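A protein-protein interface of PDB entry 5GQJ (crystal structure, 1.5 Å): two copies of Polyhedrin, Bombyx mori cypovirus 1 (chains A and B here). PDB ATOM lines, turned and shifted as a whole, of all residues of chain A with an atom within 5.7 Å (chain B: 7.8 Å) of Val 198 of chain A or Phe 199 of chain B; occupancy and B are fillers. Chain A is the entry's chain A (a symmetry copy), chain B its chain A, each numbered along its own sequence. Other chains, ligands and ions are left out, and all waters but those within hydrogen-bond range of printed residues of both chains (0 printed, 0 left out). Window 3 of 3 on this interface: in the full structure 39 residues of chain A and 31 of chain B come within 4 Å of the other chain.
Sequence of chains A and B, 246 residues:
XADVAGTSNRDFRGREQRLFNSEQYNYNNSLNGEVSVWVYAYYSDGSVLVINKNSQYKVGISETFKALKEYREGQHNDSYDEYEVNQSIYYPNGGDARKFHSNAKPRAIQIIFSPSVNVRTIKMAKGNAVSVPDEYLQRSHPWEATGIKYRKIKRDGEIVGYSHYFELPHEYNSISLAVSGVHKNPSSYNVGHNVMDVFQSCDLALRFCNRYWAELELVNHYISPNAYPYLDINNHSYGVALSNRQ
Of the 14 printed residues of chain B, 5 touch a printed residue of chain A. Printed residues of chain B that touch a printed residue of chain A: Met 196, Phe 199, Gln 200, Asp 203 and Leu 204. Hydrophobic or aromatic side chains of chain B that line the printed part of chain A: Met 196, Phe 199 and Leu 204. Among the printed residues, Asp or Glu carboxylates within 4 Å of a Lys or Arg side-chain nitrogen of the other chain: Lys 58 of chain A with Asp 203 of chain B (3.3 Å).
Lys 58 of chain A touches Phe 199 of chain B, but with the chains exchanged Phe 199 of chain A does not touch Lys 58 of chain B (6.9 Å). Val 198 of chain A touches Phe 199 of chain B, but with the chains exchanged Phe 199 of chain A does not touch Val 198 of chain B (6.9 Å). Phe 199 of chain A touches its own counterpart, Phe 199 of chain B. Cys 202 of chain A touches Phe 199 of chain B, but with the chains exchanged Phe 199 of chain A does not touch Cys 202 of chain B (6.1 Å). Positions printed for both chains: 57, 58, 194, 195, 196, 197, 198, 199, 200, 201, 202 and 203.
Among the printed residues, merely in contact across the chains: Phe 199 of chain A with Phe 199 of chain B, Val 198 of chain A with Phe 199 of chain B, Cys 202 of chain A with Phe 199 of chain B, Ser 180 of chain A with Leu 204 of chain B and Lys 58 of chain A with Met 196 of chain B.
NZ of Lys 58 of chain A sits at hydrogen-bond distance from SG of Cys 202 of chain A, at 3.6 Å. O of Val 198 of chain A sits at hydrogen-bond distance from OG of Ser 201 of chain A, at 2.6 Å. O of Val 198 of chain A sits at hydrogen-bond distance from SG of Cys 202 of chain A (3.6 Å).
O of Phe 199 of chain B sits at hydrogen-bond distance from NZ of Lys 58 of chain A. The side-chain amide oxygen (OE1) of Gln 200 of chain B is in hydrogen-bond range of the side-chain hydroxyl (OG) of Ser 180 of chain A (2.9 Å). NZ of Lys 58 of chain A is in salt-bridge range of OD1 of Asp 203 of chain B (3.3 Å). OD2 of Asp 203 of chain B is in hydrogen-bond range of OG of Ser 180 of chain A (3.3 Å).
Ser 201 of chain A touches none of the printed residues of chain B. Asp 203 of chain A touches none of the printed residues of chain B. Of the printed residues of chain A, Phe 199 of chain B touches Lys 58 (3.4 Å), Val 198 (3.6 Å), Phe 199 (3.5 Å) and Cys 202 (3.8 Å). Of the printed residues of chain A, Gln 200 of chain B touches Ser 180 (2.9 Å). Printed residues of chain A within 4 Å of Leu 204 of chain B: Ser 180. The nearest residue of chain B that does not touch Val 198 of chain A is Met 196 of chain B (4.1 Å). The nearest printed residue of chain B that does not touch Cys 202 of chain A is Cys 202 of chain B (5.6 Å).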
ATOM      1  N   TYR A  57      -4.415  -4.255   6.723  1.00  0.00           N
ATOM      2  CA  TYR A  57      -3.920  -3.094   7.522  1.00  0.00           C
ATOM      3  C   TYR A  57      -4.346  -1.708   7.024  1.00  0.00           C
ATOM      4  O   TYR A  57      -4.820  -0.894   7.809  1.00  0.00           O
ATOM      5  CB  TYR A  57      -2.381  -3.043   7.723  1.00  0.00           C
ATOM      6  CG  TYR A  57      -1.808  -4.381   8.204  1.00  0.00           C
ATOM      7  CD1 TYR A  57      -2.209  -4.921   9.442  1.00  0.00           C
ATOM      8  CD2 TYR A  57      -0.915  -5.098   7.421  1.00  0.00           C
ATOM      9  CE1 TYR A  57      -1.690  -6.143   9.871  1.00  0.00           C
ATOM     10  CE2 TYR A  57      -0.392  -6.314   7.827  1.00  0.00           C
ATOM     11  CZ  TYR A  57      -0.739  -6.793   9.077  1.00  0.00           C
ATOM     12  OH  TYR A  57      -0.222  -8.020   9.469  1.00  0.00           O
ATOM     13  N   LYS A  58      -4.088  -1.452   5.730  1.00  0.00           N
ATOM     14  CA  LYS A  58      -4.399  -0.151   5.103  1.00  0.00           C
ATOM     15  C   LYS A  58      -4.495  -0.372   3.619  1.00  0.00           C
ATOM     16  O   LYS A  58      -3.931  -1.342   3.072  1.00  0.00           O
ATOM     17  CB  LYS A  58      -3.350   0.921   5.464  1.00  0.00           C
ATOM     18  CG  LYS A  58      -1.959   0.666   4.902  1.00  0.00           C
ATOM     19  CD  LYS A  58      -1.659   1.342   3.558  1.00  0.00           C
ATOM     20  CE  LYS A  58      -0.278   0.994   3.022  1.00  0.00           C
ATOM     21  NZ  LYS A  58       0.003   1.691   1.698  1.00  0.00           N
ATOM     22  N   SER A 180      -7.382   6.789   0.692  1.00  0.00           N
ATOM     23  CA  SER A 180      -6.690   5.877   1.603  1.00  0.00           C
ATOM     24  C   SER A 180      -7.526   5.690   2.825  1.00  0.00           C
ATOM     25  O   SER A 180      -8.115   6.664   3.320  1.00  0.00           O
ATOM     26  CB  SER A 180      -5.361   6.548   2.005  1.00  0.00           C
ATOM     27  OG  SER A 180      -4.701   5.750   2.995  1.00  0.00           O
ATOM     28  N   ASN A 194       5.210  -4.978  14.201  1.00  0.00           N
ATOM     29  CA  ASN A 194       4.529  -5.479  12.989  1.00  0.00           C
ATOM     30  C   ASN A 194       4.925  -4.653  11.717  1.00  0.00           C
ATOM     31  O   ASN A 194       4.345  -4.819  10.673  1.00  0.00           O
ATOM     32  CB  ASN A 194       3.009  -5.576  13.209  1.00  0.00           C
ATOM     33  CG  ASN A 194       2.340  -6.594  12.259  1.00  0.00           C
ATOM     34  OD1 ASN A 194       2.865  -7.716  12.041  1.00  0.00           O
ATOM     35  ND2 ASN A 194       1.209  -6.192  11.664  1.00  0.00           N
ATOM     36  N   VAL A 195       5.927  -3.795  11.828  1.00  0.00           N
ATOM     37  CA  VAL A 195       6.123  -2.769  10.781  1.00  0.00           C
ATOM     38  C   VAL A 195       6.551  -3.349   9.428  1.00  0.00           C
ATOM     39  O   VAL A 195       6.051  -2.925   8.380  1.00  0.00           O
ATOM     40  CB  VAL A 195       7.125  -1.709  11.251  1.00  0.00           C
ATOM     41  CG1 VAL A 195       8.503  -2.327  11.494  1.00  0.00           C
ATOM     42  CG2 VAL A 195       7.127  -0.536  10.243  1.00  0.00           C
ATOM     43  N   MET A 196       7.446  -4.338   9.453  1.00  0.00           N
ATOM     44  CA  MET A 196       7.782  -4.985   8.202  1.00  0.00           C
ATOM     45  C   MET A 196       6.605  -5.753   7.624  1.00  0.00           C
ATOM     46  O   MET A 196       6.518  -5.853   6.377  1.00  0.00           O
ATOM     47  CB  MET A 196       9.022  -5.866   8.361  1.00  0.00           C
ATOM     48  CG  MET A 196       9.624  -6.317   7.045  1.00  0.00           C
ATOM     49  SD  MET A 196      10.163  -4.932   5.953  1.00  0.00           S
ATOM     50  CE  MET A 196      10.795  -3.820   7.225  1.00  0.00           C
ATOM     51  N   ASP A 197       5.704  -6.251   8.484  1.00  0.00           N
ATOM     52  CA  ASP A 197       4.482  -6.836   7.906  1.00  0.00           C
ATOM     53  C   ASP A 197       3.614  -5.842   7.162  1.00  0.00           C
ATOM     54  O   ASP A 197       3.028  -6.164   6.103  1.00  0.00           O
ATOM     55  CB  ASP A 197       3.630  -7.510   8.977  1.00  0.00           C
ATOM     56  CG  ASP A 197       4.220  -8.843   9.411  1.00  0.00           C
ATOM     57  OD1 ASP A 197       5.423  -8.870   9.731  1.00  0.00           O
ATOM     58  OD2 ASP A 197       3.491  -9.864   9.360  1.00  0.00           O
ATOM     59  N   VAL A 198       3.570  -4.609   7.691  1.00  0.00           N
ATOM     60  CA  VAL A 198       2.800  -3.615   6.954  1.00  0.00           C
ATOM     61  C   VAL A 198       3.511  -3.266   5.642  1.00  0.00           C
ATOM     62  O   VAL A 198       2.861  -3.100   4.599  1.00  0.00           O
ATOM     63  CB  VAL A 198       2.446  -2.361   7.820  1.00  0.00           C
ATOM     64  CG1 VAL A 198       1.551  -1.359   7.012  1.00  0.00           C
ATOM     65  CG2 VAL A 198       1.782  -2.827   9.156  1.00  0.00           C
ATOM     66  N   PHE A 199       4.852  -3.204   5.656  1.00  0.00           N
ATOM     67  CA  PHE A 199       5.583  -3.017   4.385  1.00  0.00           C
ATOM     68  C   PHE A 199       5.289  -4.132   3.409  1.00  0.00           C
ATOM     69  O   PHE A 199       5.048  -3.861   2.230  1.00  0.00           O
ATOM     70  CB  PHE A 199       7.104  -2.874   4.603  1.00  0.00           C
ATOM     71  CG  PHE A 199       7.539  -1.479   4.991  1.00  0.00           C
ATOM     72  CD1 PHE A 199       7.415  -0.436   4.089  1.00  0.00           C
ATOM     73  CD2 PHE A 199       8.057  -1.240   6.264  1.00  0.00           C
ATOM     74  CE1 PHE A 199       7.783   0.865   4.413  1.00  0.00           C
ATOM     75  CE2 PHE A 199       8.432   0.065   6.633  1.00  0.00           C
ATOM     76  CZ  PHE A 199       8.294   1.105   5.697  1.00  0.00           C
ATOM     77  N   GLN A 200       5.256  -5.389   3.847  1.00  0.00           N
ATOM     78  CA  GLN A 200       4.859  -6.474   2.909  1.00  0.00           C
ATOM     79  C   GLN A 200       3.435  -6.321   2.415  1.00  0.00           C
ATOM     80  O   GLN A 200       3.190  -6.658   1.272  1.00  0.00           O
ATOM     81  CB  GLN A 200       5.007  -7.787   3.613  1.00  0.00           C
ATOM     82  CG  GLN A 200       6.477  -8.139   3.924  1.00  0.00           C
ATOM     83  CD  GLN A 200       6.657  -9.671   4.130  1.00  0.00           C
ATOM     84  OE1 GLN A 200       6.896 -10.437   3.123  1.00  0.00           O
ATOM     85  NE2 GLN A 200       6.583 -10.085   5.347  1.00  0.00           N
ATOM     86  N   SER A 201       2.545  -5.795   3.261  1.00  0.00           N
ATOM     87  CA  SER A 201       1.158  -5.613   2.790  1.00  0.00           C
ATOM     88  C   SER A 201       1.082  -4.670   1.596  1.00  0.00           C
ATOM     89  O   SER A 201       0.180  -4.860   0.789  1.00  0.00           O
ATOM     90  CB  SER A 201       0.221  -5.124   3.918  1.00  0.00           C
ATOM     91  OG  SER A 201       0.321  -3.707   4.187  1.00  0.00           O
ATOM     92  N   CYS A 202       1.982  -3.687   1.518  1.00  0.00           N
ATOM     93  CA  CYS A 202       2.030  -2.732   0.362  1.00  0.00           C
ATOM     94  C   CYS A 202       2.320  -3.544  -0.894  1.00  0.00           C
ATOM     95  O   CYS A 202       1.808  -3.200  -1.968  1.00  0.00           O
ATOM     96  CB  CYS A 202       3.173  -1.720   0.553  1.00  0.00           C
ATOM     97  SG  CYS A 202       2.802  -0.612   1.948  1.00  0.00           S
ATOM     98  N   ASP A 203       3.145  -4.595  -0.793  1.00  0.00           N
ATOM     99  CA  ASP A 203       3.473  -5.394  -1.972  1.00  0.00           C
ATOM    100  C   ASP A 203       2.338  -6.384  -2.271  1.00  0.00           C
ATOM    101  O   ASP A 203       2.162  -6.817  -3.408  1.00  0.00           O
ATOM    102  CB  ASP A 203       4.699  -6.280  -1.679  1.00  0.00           C
ATOM    103  CG  ASP A 203       6.011  -5.538  -1.556  1.00  0.00           C
ATOM    104  OD1 ASP A 203       6.156  -4.636  -2.350  1.00  0.00           O
ATOM    105  OD2 ASP A 203       6.891  -6.065  -0.765  1.00  0.00           O
ATOM    106  N   TYR B  57       5.734  13.888   3.664  1.00  0.00           N
ATOM    107  CA  TYR B  57       6.776  13.099   4.385  1.00  0.00           C
ATOM    108  C   TYR B  57       7.970  12.636   3.542  1.00  0.00           C
ATOM    109  O   TYR B  57       9.113  12.820   3.945  1.00  0.00           O
ATOM    110  CB  TYR B  57       6.249  11.846   5.138  1.00  0.00           C
ATOM    111  CG  TYR B  57       5.031  12.159   6.014  1.00  0.00           C
ATOM    112  CD1 TYR B  57       5.138  13.072   7.081  1.00  0.00           C
ATOM    113  CD2 TYR B  57       3.797  11.579   5.753  1.00  0.00           C
ATOM    114  CE1 TYR B  57       4.024  13.357   7.870  1.00  0.00           C
ATOM    115  CE2 TYR B  57       2.678  11.854   6.521  1.00  0.00           C
ATOM    116  CZ  TYR B  57       2.820  12.694   7.611  1.00  0.00           C
ATOM    117  OH  TYR B  57       1.690  12.975   8.366  1.00  0.00           O
ATOM    118  N   LYS B  58       7.661  11.970   2.416  1.00  0.00           N
ATOM    119  CA  LYS B  58       8.693  11.423   1.512  1.00  0.00           C
ATOM    120  C   LYS B  58       8.062  11.240   0.159  1.00  0.00           C
ATOM    121  O   LYS B  58       6.827  11.119   0.032  1.00  0.00           O
ATOM    122  CB  LYS B  58       9.289  10.108   2.057  1.00  0.00           C
ATOM    123  CG  LYS B  58       8.314   8.940   2.108  1.00  0.00           C
ATOM    124  CD  LYS B  58       8.329   8.018   0.883  1.00  0.00           C
ATOM    125  CE  LYS B  58       7.288   6.910   0.970  1.00  0.00           C
ATOM    126  NZ  LYS B  58       7.336   5.998  -0.248  1.00  0.00           N
ATOM    127  N   ASN B 194       3.569   8.136  14.214  1.00  0.00           N
ATOM    128  CA  ASN B 194       3.031   8.648  12.937  1.00  0.00           C
ATOM    129  C   ASN B 194       3.157   7.588  11.789  1.00  0.00           C
ATOM    130  O   ASN B 194       2.916   7.891  10.646  1.00  0.00           O
ATOM    131  CB  ASN B 194       3.648  10.012  12.583  1.00  0.00           C
ATOM    132  CG  ASN B 194       2.750  10.837  11.635  1.00  0.00           C
ATOM    133  OD1 ASN B 194       1.507  10.906  11.819  1.00  0.00           O
ATOM    134  ND2 ASN B 194       3.366  11.425  10.601  1.00  0.00           N
ATOM    135  N   VAL B 195       3.509   6.356  12.123  1.00  0.00           N
ATOM    136  CA  VAL B 195       3.961   5.420  11.072  1.00  0.00           C
ATOM    137  C   VAL B 195       2.851   5.015  10.094  1.00  0.00           C
ATOM    138  O   VAL B 195       3.078   4.956   8.881  1.00  0.00           O
ATOM    139  CB  VAL B 195       4.601   4.178  11.700  1.00  0.00           C
ATOM    140  CG1 VAL B 195       3.584   3.403  12.541  1.00  0.00           C
ATOM    141  CG2 VAL B 195       5.271   3.338  10.587  1.00  0.00           C
ATOM    142  N   MET B 196       1.648   4.772  10.616  1.00  0.00           N
ATOM    143  CA  MET B 196       0.552   4.502   9.710  1.00  0.00           C
ATOM    144  C   MET B 196       0.197   5.717   8.868  1.00  0.00           C
ATOM    145  O   MET B 196      -0.256   5.527   7.714  1.00  0.00           O
ATOM    146  CB  MET B 196      -0.658   3.953  10.465  1.00  0.00           C
ATOM    147  CG  MET B 196      -1.718   3.349   9.566  1.00  0.00           C
ATOM    148  SD  MET B 196      -1.117   1.937   8.541  1.00  0.00           S
ATOM    149  CE  MET B 196      -0.019   1.176   9.754  1.00  0.00           C
ATOM    150  N   ASP B 197       0.425   6.929   9.397  1.00  0.00           N
ATOM    151  CA  ASP B 197       0.245   8.090   8.509  1.00  0.00           C
ATOM    152  C   ASP B 197       1.208   8.128   7.339  1.00  0.00           C
ATOM    153  O   ASP B 197       0.832   8.510   6.207  1.00  0.00           O
ATOM    154  CB  ASP B 197       0.371   9.401   9.278  1.00  0.00           C
ATOM    155  CG  ASP B 197      -0.865   9.685  10.115  1.00  0.00           C
ATOM    156  OD1 ASP B 197      -1.281   8.781  10.863  1.00  0.00           O
ATOM    157  OD2 ASP B 197      -1.449  10.787   9.964  1.00  0.00           O
ATOM    158  N   VAL B 198       2.447   7.682   7.601  1.00  0.00           N
ATOM    159  CA  VAL B 198       3.371   7.640   6.475  1.00  0.00           C
ATOM    160  C   VAL B 198       2.949   6.548   5.487  1.00  0.00           C
ATOM    161  O   VAL B 198       3.020   6.742   4.264  1.00  0.00           O
ATOM    162  CB  VAL B 198       4.866   7.525   6.924  1.00  0.00           C
ATOM    163  CG1 VAL B 198       5.826   7.566   5.685  1.00  0.00           C
ATOM    164  CG2 VAL B 198       5.178   8.644   7.971  1.00  0.00           C
ATOM    165  N   PHE B 199       2.452   5.408   5.992  1.00  0.00           N
ATOM    166  CA  PHE B 199       1.896   4.389   5.077  1.00  0.00           C
ATOM    167  C   PHE B 199       0.752   4.945   4.261  1.00  0.00           C
ATOM    168  O   PHE B 199       0.699   4.714   3.051  1.00  0.00           O
ATOM    169  CB  PHE B 199       1.459   3.110   5.823  1.00  0.00           C
ATOM    170  CG  PHE B 199       2.592   2.151   6.108  1.00  0.00           C
ATOM    171  CD1 PHE B 199       3.239   1.508   5.066  1.00  0.00           C
ATOM    172  CD2 PHE B 199       2.996   1.921   7.424  1.00  0.00           C
ATOM    173  CE1 PHE B 199       4.298   0.635   5.283  1.00  0.00           C
ATOM    174  CE2 PHE B 199       4.070   1.051   7.684  1.00  0.00           C
ATOM    175  CZ  PHE B 199       4.708   0.412   6.606  1.00  0.00           C
ATOM    176  N   GLN B 200      -0.161   5.709   4.857  1.00  0.00           N
ATOM    177  CA  GLN B 200      -1.225   6.344   4.032  1.00  0.00           C
ATOM    178  C   GLN B 200      -0.667   7.326   3.022  1.00  0.00           C
ATOM    179  O   GLN B 200      -1.223   7.411   1.944  1.00  0.00           O
ATOM    180  CB  GLN B 200      -2.175   7.053   4.948  1.00  0.00           C
ATOM    181  CG  GLN B 200      -2.981   6.086   5.841  1.00  0.00           C
ATOM    182  CD  GLN B 200      -4.291   6.753   6.350  1.00  0.00           C
ATOM    183  OE1 GLN B 200      -5.369   6.684   5.649  1.00  0.00           O
ATOM    184  NE2 GLN B 200      -4.218   7.325   7.501  1.00  0.00           N
ATOM    185  N   SER B 201       0.423   8.013   3.372  1.00  0.00           N
ATOM    186  CA  SER B 201       0.998   8.956   2.393  1.00  0.00           C
ATOM    187  C   SER B 201       1.444   8.250   1.119  1.00  0.00           C
ATOM    188  O   SER B 201       1.394   8.891   0.076  1.00  0.00           O
ATOM    189  CB  SER B 201       2.168   9.772   2.989  1.00  0.00           C
ATOM    190  OG  SER B 201       3.419   9.050   3.036  1.00  0.00           O
ATOM    191  N   CYS B 202       1.883   6.994   1.222  1.00  0.00           N
ATOM    192  CA  CYS B 202       2.301   6.187   0.028  1.00  0.00           C
ATOM    193  C   CYS B 202       1.082   6.038  -0.874  1.00  0.00           C
ATOM    194  O   CYS B 202       1.238   6.021  -2.103  1.00  0.00           O
ATOM    195  CB  CYS B 202       2.751   4.782   0.463  1.00  0.00           C
ATOM    196  SG  CYS B 202       4.300   4.887   1.412  1.00  0.00           S
ATOM    197  N   ASP B 203      -0.120   5.902  -0.299  1.00  0.00           N
ATOM    198  CA  ASP B 203      -1.318   5.733  -1.119  1.00  0.00           C
ATOM    199  C   ASP B 203      -1.788   7.093  -1.653  1.00  0.00           C
ATOM    200  O   ASP B 203      -2.454   7.171  -2.684  1.00  0.00           O
ATOM    201  CB  ASP B 203      -2.484   5.231  -0.244  1.00  0.00           C
ATOM    202  CG  ASP B 203      -2.355   3.803   0.237  1.00  0.00           C
ATOM    203  OD1 ASP B 203      -1.905   3.033  -0.582  1.00  0.00           O
ATOM    204  OD2 ASP B 203      -2.910   3.534   1.376  1.00  0.00           O
ATOM    205  N   LEU B 204      -1.567   8.162  -0.880  1.00  0.00           N
ATOM    206  CA  LEU B 204      -2.147   9.490  -1.162  1.00  0.00           C
ATOM    207  C   LEU B 204      -1.329  10.335  -2.146  1.00  0.00           C
ATOM    208  O   LEU B 204      -1.825  11.334  -2.671  1.00  0.00           O
ATOM    209  CB  LEU B 204      -2.334  10.255   0.152  1.00  0.00           C
ATOM    210  CG  LEU B 204      -3.494   9.708   1.015  1.00  0.00           C
ATOM    211  CD1 LEU B 204      -3.366  10.175   2.489  1.00  0.00           C
ATOM    212  CD2 LEU B 204      -4.894   9.986   0.449  1.00  0.00           C
ATOM    213  N   ALA B 205      -0.094   9.863  -2.375  1.00  0.00           N
ATOM    214  CA  ALA B 205       0.851  10.618  -3.245  1.00  0.00           C
ATOM    215  C   ALA B 205       0.143  10.763  -4.584  1.00  0.00           C
ATOM    216  O   ALA B 205      -0.383   9.789  -5.108  1.00  0.00           O
ATOM    217  CB  ALA B 205       2.192   9.918  -3.357  1.00  0.00           C
